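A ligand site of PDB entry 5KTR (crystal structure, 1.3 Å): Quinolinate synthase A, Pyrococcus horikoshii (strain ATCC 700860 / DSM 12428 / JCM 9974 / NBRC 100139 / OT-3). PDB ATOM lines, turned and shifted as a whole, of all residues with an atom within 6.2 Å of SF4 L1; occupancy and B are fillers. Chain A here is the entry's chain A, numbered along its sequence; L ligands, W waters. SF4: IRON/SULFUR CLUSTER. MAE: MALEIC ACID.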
ATOM      1  N   HIS A  25     -18.741  13.098   7.353  1.00  0.00           N
ATOM      2  CA  HIS A  25     -18.551  12.036   6.391  1.00  0.00           C
ATOM      3  C   HIS A  25     -17.959  12.592   5.087  1.00  0.00           C
ATOM      4  O   HIS A  25     -18.136  13.771   4.729  1.00  0.00           O
ATOM      5  CB  HIS A  25     -19.870  11.314   6.090  1.00  0.00           C
ATOM      6  CG  HIS A  25     -19.677  10.101   5.255  1.00  0.00           C
ATOM      7  ND1 HIS A  25     -19.847  10.105   3.889  1.00  0.00           N
ATOM      8  CD2 HIS A  25     -19.266   8.847   5.587  1.00  0.00           C
ATOM      9  CE1 HIS A  25     -19.574   8.899   3.414  1.00  0.00           C
ATOM     10  NE2 HIS A  25     -19.201   8.126   4.425  1.00  0.00           N
ATOM     11  N   TYR A  27     -18.936  12.314   2.149  1.00  0.00           N
ATOM     12  CA  TYR A  27     -19.900  12.794   1.157  1.00  0.00           C
ATOM     13  C   TYR A  27     -20.463  14.163   1.485  1.00  0.00           C
ATOM     14  O   TYR A  27     -21.371  14.628   0.788  1.00  0.00           O
ATOM     15  CB  TYR A  27     -21.096  11.826   1.017  1.00  0.00           C
ATOM     16  CG  TYR A  27     -20.769  10.407   0.588  1.00  0.00           C
ATOM     17  CD1 TYR A  27     -19.585  10.095  -0.065  1.00  0.00           C
ATOM     18  CD2 TYR A  27     -21.652   9.365   0.850  1.00  0.00           C
ATOM     19  CE1 TYR A  27     -19.286   8.787  -0.441  1.00  0.00           C
ATOM     20  CE2 TYR A  27     -21.360   8.046   0.493  1.00  0.00           C
ATOM     21  CZ  TYR A  27     -20.186   7.762  -0.158  1.00  0.00           C
ATOM     22  OH  TYR A  27     -19.903   6.458  -0.515  1.00  0.00           O
ATOM     23  N   VAL A  62     -25.427  11.417   8.189  1.00  0.00           N
ATOM     24  CA  VAL A  62     -26.814  10.979   8.309  1.00  0.00           C
ATOM     25  C   VAL A  62     -27.136  10.483   9.705  1.00  0.00           C
ATOM     26  O   VAL A  62     -26.239  10.209  10.515  1.00  0.00           O
ATOM     27  CB  VAL A  62     -27.180   9.945   7.220  1.00  0.00           C
ATOM     28  CG1 VAL A  62     -27.103  10.611   5.844  1.00  0.00           C
ATOM     29  CG2 VAL A  62     -26.254   8.743   7.282  1.00  0.00           C
ATOM     30  N   PHE A  64     -28.177   7.721  11.129  1.00  0.00           N
ATOM     31  CA  PHE A  64     -27.625   6.462  11.650  1.00  0.00           C
ATOM     32  C   PHE A  64     -26.189   6.657  12.138  1.00  0.00           C
ATOM     33  O   PHE A  64     -25.794   6.085  13.154  1.00  0.00           O
ATOM     34  CB  PHE A  64     -27.807   5.272  10.677  1.00  0.00           C
ATOM     35  CG  PHE A  64     -26.806   5.196   9.509  1.00  0.00           C
ATOM     36  CD1 PHE A  64     -25.487   4.826   9.705  1.00  0.00           C
ATOM     37  CD2 PHE A  64     -27.230   5.406   8.198  1.00  0.00           C
ATOM     38  CE1 PHE A  64     -24.603   4.735   8.640  1.00  0.00           C
ATOM     39  CE2 PHE A  64     -26.358   5.307   7.135  1.00  0.00           C
ATOM     40  CZ  PHE A  64     -25.036   4.981   7.365  1.00  0.00           C
ATOM     41  N   MET A  65     -25.428   7.505  11.445  1.00  0.00           N
ATOM     42  CA  MET A  65     -24.059   7.768  11.858  1.00  0.00           C
ATOM     43  C   MET A  65     -24.027   8.552  13.164  1.00  0.00           C
ATOM     44  O   MET A  65     -23.228   8.254  14.051  1.00  0.00           O
ATOM     45  CB  MET A  65     -23.332   8.562  10.786  1.00  0.00           C
ATOM     46  CG  MET A  65     -23.166   7.820   9.492  1.00  0.00           C
ATOM     47  SD  MET A  65     -22.416   8.860   8.224  1.00  0.00           S
ATOM     48  CE  MET A  65     -22.343   7.620   6.919  1.00  0.00           C
ATOM     49  N   THR A  86     -30.966  11.460   6.367  1.00  0.00           N
ATOM     50  CA  THR A  86     -31.209  10.052   6.646  1.00  0.00           C
ATOM     51  C   THR A  86     -30.824   9.210   5.437  1.00  0.00           C
ATOM     52  O   THR A  86     -30.659   9.711   4.319  1.00  0.00           O
ATOM     53  CB  THR A  86     -32.644   9.779   7.097  1.00  0.00           C
ATOM     54  OG1 THR A  86     -32.723   8.469   7.686  1.00  0.00           O
ATOM     55  CG2 THR A  86     -33.600   9.858   5.922  1.00  0.00           C
ATOM     56  N   CYS A  87     -30.704   7.918   5.684  1.00  0.00           N
ATOM     57  CA  CYS A  87     -30.156   6.954   4.736  1.00  0.00           C
ATOM     58  C   CYS A  87     -31.259   6.043   4.235  1.00  0.00           C
ATOM     59  O   CYS A  87     -31.852   5.278   5.015  1.00  0.00           O
ATOM     60  CB  CYS A  87     -29.046   6.144   5.383  1.00  0.00           C
ATOM     61  SG  CYS A  87     -28.409   4.789   4.400  1.00  0.00           S
ATOM     62  N   ALA A  88     -31.484   6.067   2.917  1.00  0.00           N
ATOM     63  CA  ALA A  88     -32.535   5.248   2.332  1.00  0.00           C
ATOM     64  C   ALA A  88     -32.198   3.760   2.445  1.00  0.00           C
ATOM     65  O   ALA A  88     -33.077   2.943   2.704  1.00  0.00           O
ATOM     66  CB  ALA A  88     -32.786   5.649   0.876  1.00  0.00           C
ATOM     67  N   MET A  89     -30.926   3.384   2.276  1.00  0.00           N
ATOM     68  CA  MET A  89     -30.567   1.973   2.368  1.00  0.00           C
ATOM     69  C   MET A  89     -30.823   1.431   3.774  1.00  0.00           C
ATOM     70  O   MET A  89     -31.416   0.361   3.933  1.00  0.00           O
ATOM     71  CB  MET A  89     -29.128   1.738   1.889  1.00  0.00           C
ATOM     72  CG  MET A  89     -28.661   0.240   1.882  1.00  0.00           C
ATOM     73  SD  MET A  89     -27.684  -0.022   3.396  1.00  0.00           S
ATOM     74  CE  MET A  89     -26.219   0.812   2.797  1.00  0.00           C
ATOM     75  N   ALA A  90     -30.438   2.187   4.808  1.00  0.00           N
ATOM     76  CA  ALA A  90     -30.575   1.731   6.188  1.00  0.00           C
ATOM     77  C   ALA A  90     -32.044   1.581   6.573  1.00  0.00           C
ATOM     78  O   ALA A  90     -32.401   0.660   7.333  1.00  0.00           O
ATOM     79  CB  ALA A  90     -29.927   2.758   7.108  1.00  0.00           C
ATOM     80  N   TYR A 113     -24.668  -4.066   8.718  1.00  0.00           N
ATOM     81  CA  TYR A 113     -24.030  -2.893   8.194  1.00  0.00           C
ATOM     82  C   TYR A 113     -24.403  -1.730   9.091  1.00  0.00           C
ATOM     83  O   TYR A 113     -25.525  -1.658   9.590  1.00  0.00           O
ATOM     84  CB  TYR A 113     -24.593  -2.670   6.789  1.00  0.00           C
ATOM     85  CG  TYR A 113     -23.744  -1.872   5.833  1.00  0.00           C
ATOM     86  CD1 TYR A 113     -24.280  -1.426   4.630  1.00  0.00           C
ATOM     87  CD2 TYR A 113     -22.411  -1.583   6.096  1.00  0.00           C
ATOM     88  CE1 TYR A 113     -23.532  -0.716   3.744  1.00  0.00           C
ATOM     89  CE2 TYR A 113     -21.659  -0.857   5.199  1.00  0.00           C
ATOM     90  CZ  TYR A 113     -22.226  -0.418   4.030  1.00  0.00           C
ATOM     91  OH  TYR A 113     -21.478   0.306   3.147  1.00  0.00           O
ATOM     92  N   ASN A 115     -25.026   1.077   8.251  1.00  0.00           N
ATOM     93  CA  ASN A 115     -26.187   1.700   7.630  1.00  0.00           C
ATOM     94  C   ASN A 115     -27.423   0.929   8.074  1.00  0.00           C
ATOM     95  O   ASN A 115     -27.997   0.128   7.342  1.00  0.00           O
ATOM     96  CB  ASN A 115     -26.080   1.682   6.106  1.00  0.00           C
ATOM     97  CG  ASN A 115     -24.773   2.245   5.586  1.00  0.00           C
ATOM     98  OD1 ASN A 115     -23.709   1.967   6.123  1.00  0.00           O
ATOM     99  ND2 ASN A 115     -24.855   3.031   4.519  1.00  0.00           N
ATOM    100  N   ASP A 150     -27.433  -4.098   2.835  1.00  0.00           N
ATOM    101  CA  ASP A 150     -27.075  -3.849   1.441  1.00  0.00           C
ATOM    102  C   ASP A 150     -26.752  -5.150   0.711  1.00  0.00           C
ATOM    103  O   ASP A 150     -25.777  -5.831   1.040  1.00  0.00           O
ATOM    104  CB  ASP A 150     -25.919  -2.863   1.338  1.00  0.00           C
ATOM    105  CG  ASP A 150     -25.702  -2.375  -0.055  1.00  0.00           C
ATOM    106  OD1 ASP A 150     -26.080  -1.224  -0.347  1.00  0.00           O
ATOM    107  OD2 ASP A 150     -25.177  -3.155  -0.886  1.00  0.00           O
ATOM    108  N   CYS A 174     -28.500   0.910  -2.038  1.00  0.00           N
ATOM    109  CA  CYS A 174     -28.322   2.356  -2.026  1.00  0.00           C
ATOM    110  C   CYS A 174     -28.603   2.910  -3.420  1.00  0.00           C
ATOM    111  O   CYS A 174     -27.904   2.571  -4.379  1.00  0.00           O
ATOM    112  CB  CYS A 174     -26.878   2.682  -1.637  1.00  0.00           C
ATOM    113  SG  CYS A 174     -26.414   4.395  -1.952  1.00  0.00           S
ATOM    114  N   TYR A 175     -29.619   3.776  -3.539  1.00  0.00           N
ATOM    115  CA  TYR A 175     -29.975   4.322  -4.860  1.00  0.00           C
ATOM    116  C   TYR A 175     -28.841   5.118  -5.482  1.00  0.00           C
ATOM    117  O   TYR A 175     -28.752   5.209  -6.716  1.00  0.00           O
ATOM    118  CB  TYR A 175     -31.243   5.200  -4.768  1.00  0.00           C
ATOM    119  CG  TYR A 175     -31.060   6.496  -4.014  1.00  0.00           C
ATOM    120  CD1 TYR A 175     -30.735   7.672  -4.682  1.00  0.00           C
ATOM    121  CD2 TYR A 175     -31.204   6.554  -2.636  1.00  0.00           C
ATOM    122  CE1 TYR A 175     -30.580   8.874  -3.996  1.00  0.00           C
ATOM    123  CE2 TYR A 175     -31.032   7.747  -1.939  1.00  0.00           C
ATOM    124  CZ  TYR A 175     -30.721   8.899  -2.632  1.00  0.00           C
ATOM    125  OH  TYR A 175     -30.553  10.090  -1.959  1.00  0.00           O
ATOM    126  N   VAL A 176     -27.981   5.733  -4.662  1.00  0.00           N
ATOM    127  CA  VAL A 176     -26.855   6.501  -5.194  1.00  0.00           C
ATOM    128  C   VAL A 176     -25.933   5.588  -5.981  1.00  0.00           C
ATOM    129  O   VAL A 176     -25.583   5.851  -7.138  1.00  0.00           O
ATOM    130  CB  VAL A 176     -26.102   7.222  -4.066  1.00  0.00           C
ATOM    131  CG1 VAL A 176     -24.969   8.059  -4.642  1.00  0.00           C
ATOM    132  CG2 VAL A 176     -27.062   8.075  -3.237  1.00  0.00           C
ATOM    133  N   HIS A 177     -25.508   4.486  -5.352  1.00  0.00           N
ATOM    134  CA  HIS A 177     -24.559   3.576  -5.985  1.00  0.00           C
ATOM    135  C   HIS A 177     -25.197   2.702  -7.042  1.00  0.00           C
ATOM    136  O   HIS A 177     -24.487   2.266  -7.958  1.00  0.00           O
ATOM    137  CB  HIS A 177     -23.840   2.747  -4.921  1.00  0.00           C
ATOM    138  CG  HIS A 177     -22.896   3.562  -4.091  1.00  0.00           C
ATOM    139  ND1 HIS A 177     -23.292   4.189  -2.926  1.00  0.00           N
ATOM    140  CD2 HIS A 177     -21.612   3.921  -4.306  1.00  0.00           C
ATOM    141  CE1 HIS A 177     -22.261   4.879  -2.444  1.00  0.00           C
ATOM    142  NE2 HIS A 177     -21.238   4.725  -3.258  1.00  0.00           N
ATOM    143  N   GLU A 202     -21.052  -0.976  -2.659  1.00  0.00           N
ATOM    144  CA  GLU A 202     -22.493  -0.798  -2.807  1.00  0.00           C
ATOM    145  C   GLU A 202     -22.922  -0.714  -4.269  1.00  0.00           C
ATOM    146  O   GLU A 202     -24.125  -0.683  -4.541  1.00  0.00           O
ATOM    147  CB  GLU A 202     -22.962   0.428  -2.027  1.00  0.00           C
ATOM    148  CG  GLU A 202     -22.934   0.238  -0.512  1.00  0.00           C
ATOM    149  CD  GLU A 202     -23.270   1.503   0.251  1.00  0.00           C
ATOM    150  OE1 GLU A 202     -23.913   2.392  -0.327  1.00  0.00           O
ATOM    151  OE2 GLU A 202     -22.900   1.625   1.436  1.00  0.00           O
ATOM    152  N   GLU A 235     -20.405   8.418  -4.377  1.00  0.00           N
ATOM    153  CA  GLU A 235     -21.090   9.702  -4.320  1.00  0.00           C
ATOM    154  C   GLU A 235     -20.117  10.826  -4.687  1.00  0.00           C
ATOM    155  O   GLU A 235     -18.971  10.837  -4.249  1.00  0.00           O
ATOM    156  CB  GLU A 235     -21.606   9.909  -2.892  1.00  0.00           C
ATOM    157  CG  GLU A 235     -22.875  10.716  -2.741  1.00  0.00           C
ATOM    158  CD  GLU A 235     -22.643  12.217  -2.654  1.00  0.00           C
ATOM    159  OE1 GLU A 235     -23.661  12.956  -2.589  1.00  0.00           O
ATOM    160  OE2 GLU A 235     -21.488  12.668  -2.632  1.00  0.00           O
ATOM    161  N   CYS A 260     -26.258  11.929  -2.819  1.00  0.00           N
ATOM    162  CA  CYS A 260     -27.072  11.450  -1.698  1.00  0.00           C
ATOM    163  C   CYS A 260     -27.850  12.633  -1.117  1.00  0.00           C
ATOM    164  O   CYS A 260     -27.264  13.540  -0.502  1.00  0.00           O
ATOM    165  CB  CYS A 260     -26.200  10.812  -0.612  1.00  0.00           C
ATOM    166  SG  CYS A 260     -27.203  10.288   0.810  1.00  0.00           S
ATOM    167  N   ILE A 261     -29.168  12.616  -1.300  1.00  0.00           N
ATOM    168  CA  ILE A 261     -30.016  13.691  -0.788  1.00  0.00           C
ATOM    169  C   ILE A 261     -29.882  13.806   0.722  1.00  0.00           C
ATOM    170  O   ILE A 261     -29.840  14.908   1.274  1.00  0.00           O
ATOM    171  CB  ILE A 261     -31.470  13.490  -1.252  1.00  0.00           C
ATOM    172  CG1 ILE A 261     -31.566  13.545  -2.780  1.00  0.00           C
ATOM    173  CG2 ILE A 261     -32.397  14.533  -0.628  1.00  0.00           C
ATOM    174  CD1 ILE A 261     -32.953  13.320  -3.334  1.00  0.00           C
ATOM    175  N   GLY A 262     -29.817  12.673   1.426  1.00  0.00           N
ATOM    176  CA  GLY A 262     -29.734  12.735   2.885  1.00  0.00           C
ATOM    177  C   GLY A 262     -28.466  13.408   3.378  1.00  0.00           C
ATOM    178  O   GLY A 262     -28.512  14.240   4.298  1.00  0.00           O
ATOM    179  N   MET A 263     -27.332  13.069   2.778  1.00  0.00           N
ATOM    180  CA  MET A 263     -26.086  13.736   3.134  1.00  0.00           C
ATOM    181  C   MET A 263     -26.193  15.238   2.923  1.00  0.00           C
ATOM    182  O   MET A 263     -25.701  16.024   3.755  1.00  0.00           O
ATOM    183  CB  MET A 263     -24.935  13.161   2.291  1.00  0.00           C
ATOM    184  CG  MET A 263     -24.500  11.777   2.754  1.00  0.00           C
ATOM    185  SD  MET A 263     -23.627  11.847   4.339  1.00  0.00           S
ATOM    186  CE  MET A 263     -23.323  10.101   4.604  1.00  0.00           C
HETATM  187 FE1  SF4 L   1     -27.395   5.808   2.575  1.00  0.00          FE
HETATM  188 FE2  SF4 L   1     -26.792   8.065   1.202  1.00  0.00          FE
HETATM  189 FE3  SF4 L   1     -26.490   5.599   0.041  1.00  0.00          FE
HETATM  190 FE4  SF4 L   1     -24.883   6.329   2.112  1.00  0.00          FE
HETATM  191  S1  SF4 L   1     -24.997   7.290   0.020  1.00  0.00           S
HETATM  192  S2  SF4 L   1     -25.896   4.280   1.784  1.00  0.00           S
HETATM  193  S3  SF4 L   1     -26.333   7.615   3.374  1.00  0.00           S
HETATM  194  S4  SF4 L   1     -28.473   6.539   0.707  1.00  0.00           S
HETATM  195  C1  MAE L   2     -19.037   2.793   4.833  1.00  0.00           C
HETATM  196  O1  MAE L   2     -17.925   3.220   5.093  1.00  0.00           O
HETATM  197  O2  MAE L   2     -19.378   1.555   5.194  1.00  0.00           O
HETATM  198  C2  MAE L   2     -20.057   3.593   4.130  1.00  0.00           C
HETATM  199  C3  MAE L   2     -19.718   4.524   3.222  1.00  0.00           C
HETATM  200  C4  MAE L   2     -18.322   4.847   2.875  1.00  0.00           C
HETATM  201  O3  MAE L   2     -17.842   5.968   3.405  1.00  0.00           O
HETATM  202  O4  MAE L   2     -17.633   4.160   2.147  1.00  0.00           O
HETATM  203  O   HOH W   1     -22.204   4.704   0.904  1.00  0.00           O
HETATM  204  O   HOH W   2     -30.779   8.902   1.750  1.00  0.00           O
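The side-chain amide nitrogen (ND2) of Asn 115 sits close to a sulfur (S2) of SF4 L1 (3.2 Å).
The side-chain sulfur of Cys 260 is bound to an iron atom (FE2) of SF4 L1 (2.3 Å).
SG of Cys 174 binds FE3 of SF4 L1 (2.3 Å).
O2 of MAE L2 lies within hydrogen-bond range of OH of Tyr 113.
An iron atom (FE1) of SF4 L1 is bound by the side-chain sulfur (SG) of Cys 87.
A ring nitrogen (NE2) of His 25 is in hydrogen-bond range of an oxygen (O3) of MAE L2 (2.7 Å).
N of Ala 88 sits close to S4 of SF4 L1 (3.8 Å).
SG of Cys 87 sits close to N of Ala 90 (3.3 Å).
The side-chain carboxylate of Glu 202 sits at hydrogen-bond distance from a ring nitrogen (ND1) of His 177, 3.2 Å away.
The side-chain sulfur (SG) of Cys 174 lies close to the side-chain carboxylate (OE1) of Glu 202, at 3.6 Å.
A ring nitrogen (ND1) of His 25 lies within hydrogen-bond range of the backbone NH (N) of Tyr 27 (3.0 Å).
OH of Tyr 175 is in hydrogen-bond range of N of Ile 261, 3.0 Å away.
SG of Cys 260 lies close to N of Gly 262 (3.6 Å).
N of Met 89 lies close to SG of Cys 87, 3.6 Å away.
SG of Cys 174 sits close to N of Val 176, at 3.4 Å.
Water W1 bridges OE1 of Glu 202 and OH of Tyr 27.
Water W2 lies within hydrogen-bond range of the backbone carbonyl oxygen (O) of Thr 86 (2.7 Å), the backbone NH (N) of Ala 88 (3.1 Å) and a sulfur (S4) of SF4 L1 (3.5 Å).
The side-chain carboxylate (OE1) of Glu 202 sits close to a sulfur (S2) of SF4 L1, at 3.5 Å.
Tyr 27 touches SF4 L1.
Val 62 touches SF4 L1.
Met 89 touches SF4 L1.
CE2 of Tyr 175 touches S4 of SF4 L1 (3.9 Å).
Val 176 touches SF4 L1 (CG2 to S1, 3.9 Å).
Hydrophobic or aromatic side chains within 4 Å of SF4 L1: Tyr 27, Val 62, Met 89, Tyr 175 and Val 176.
The nearest printed residue that does not touch SF4 L1 is Met 263 (4.1 Å).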
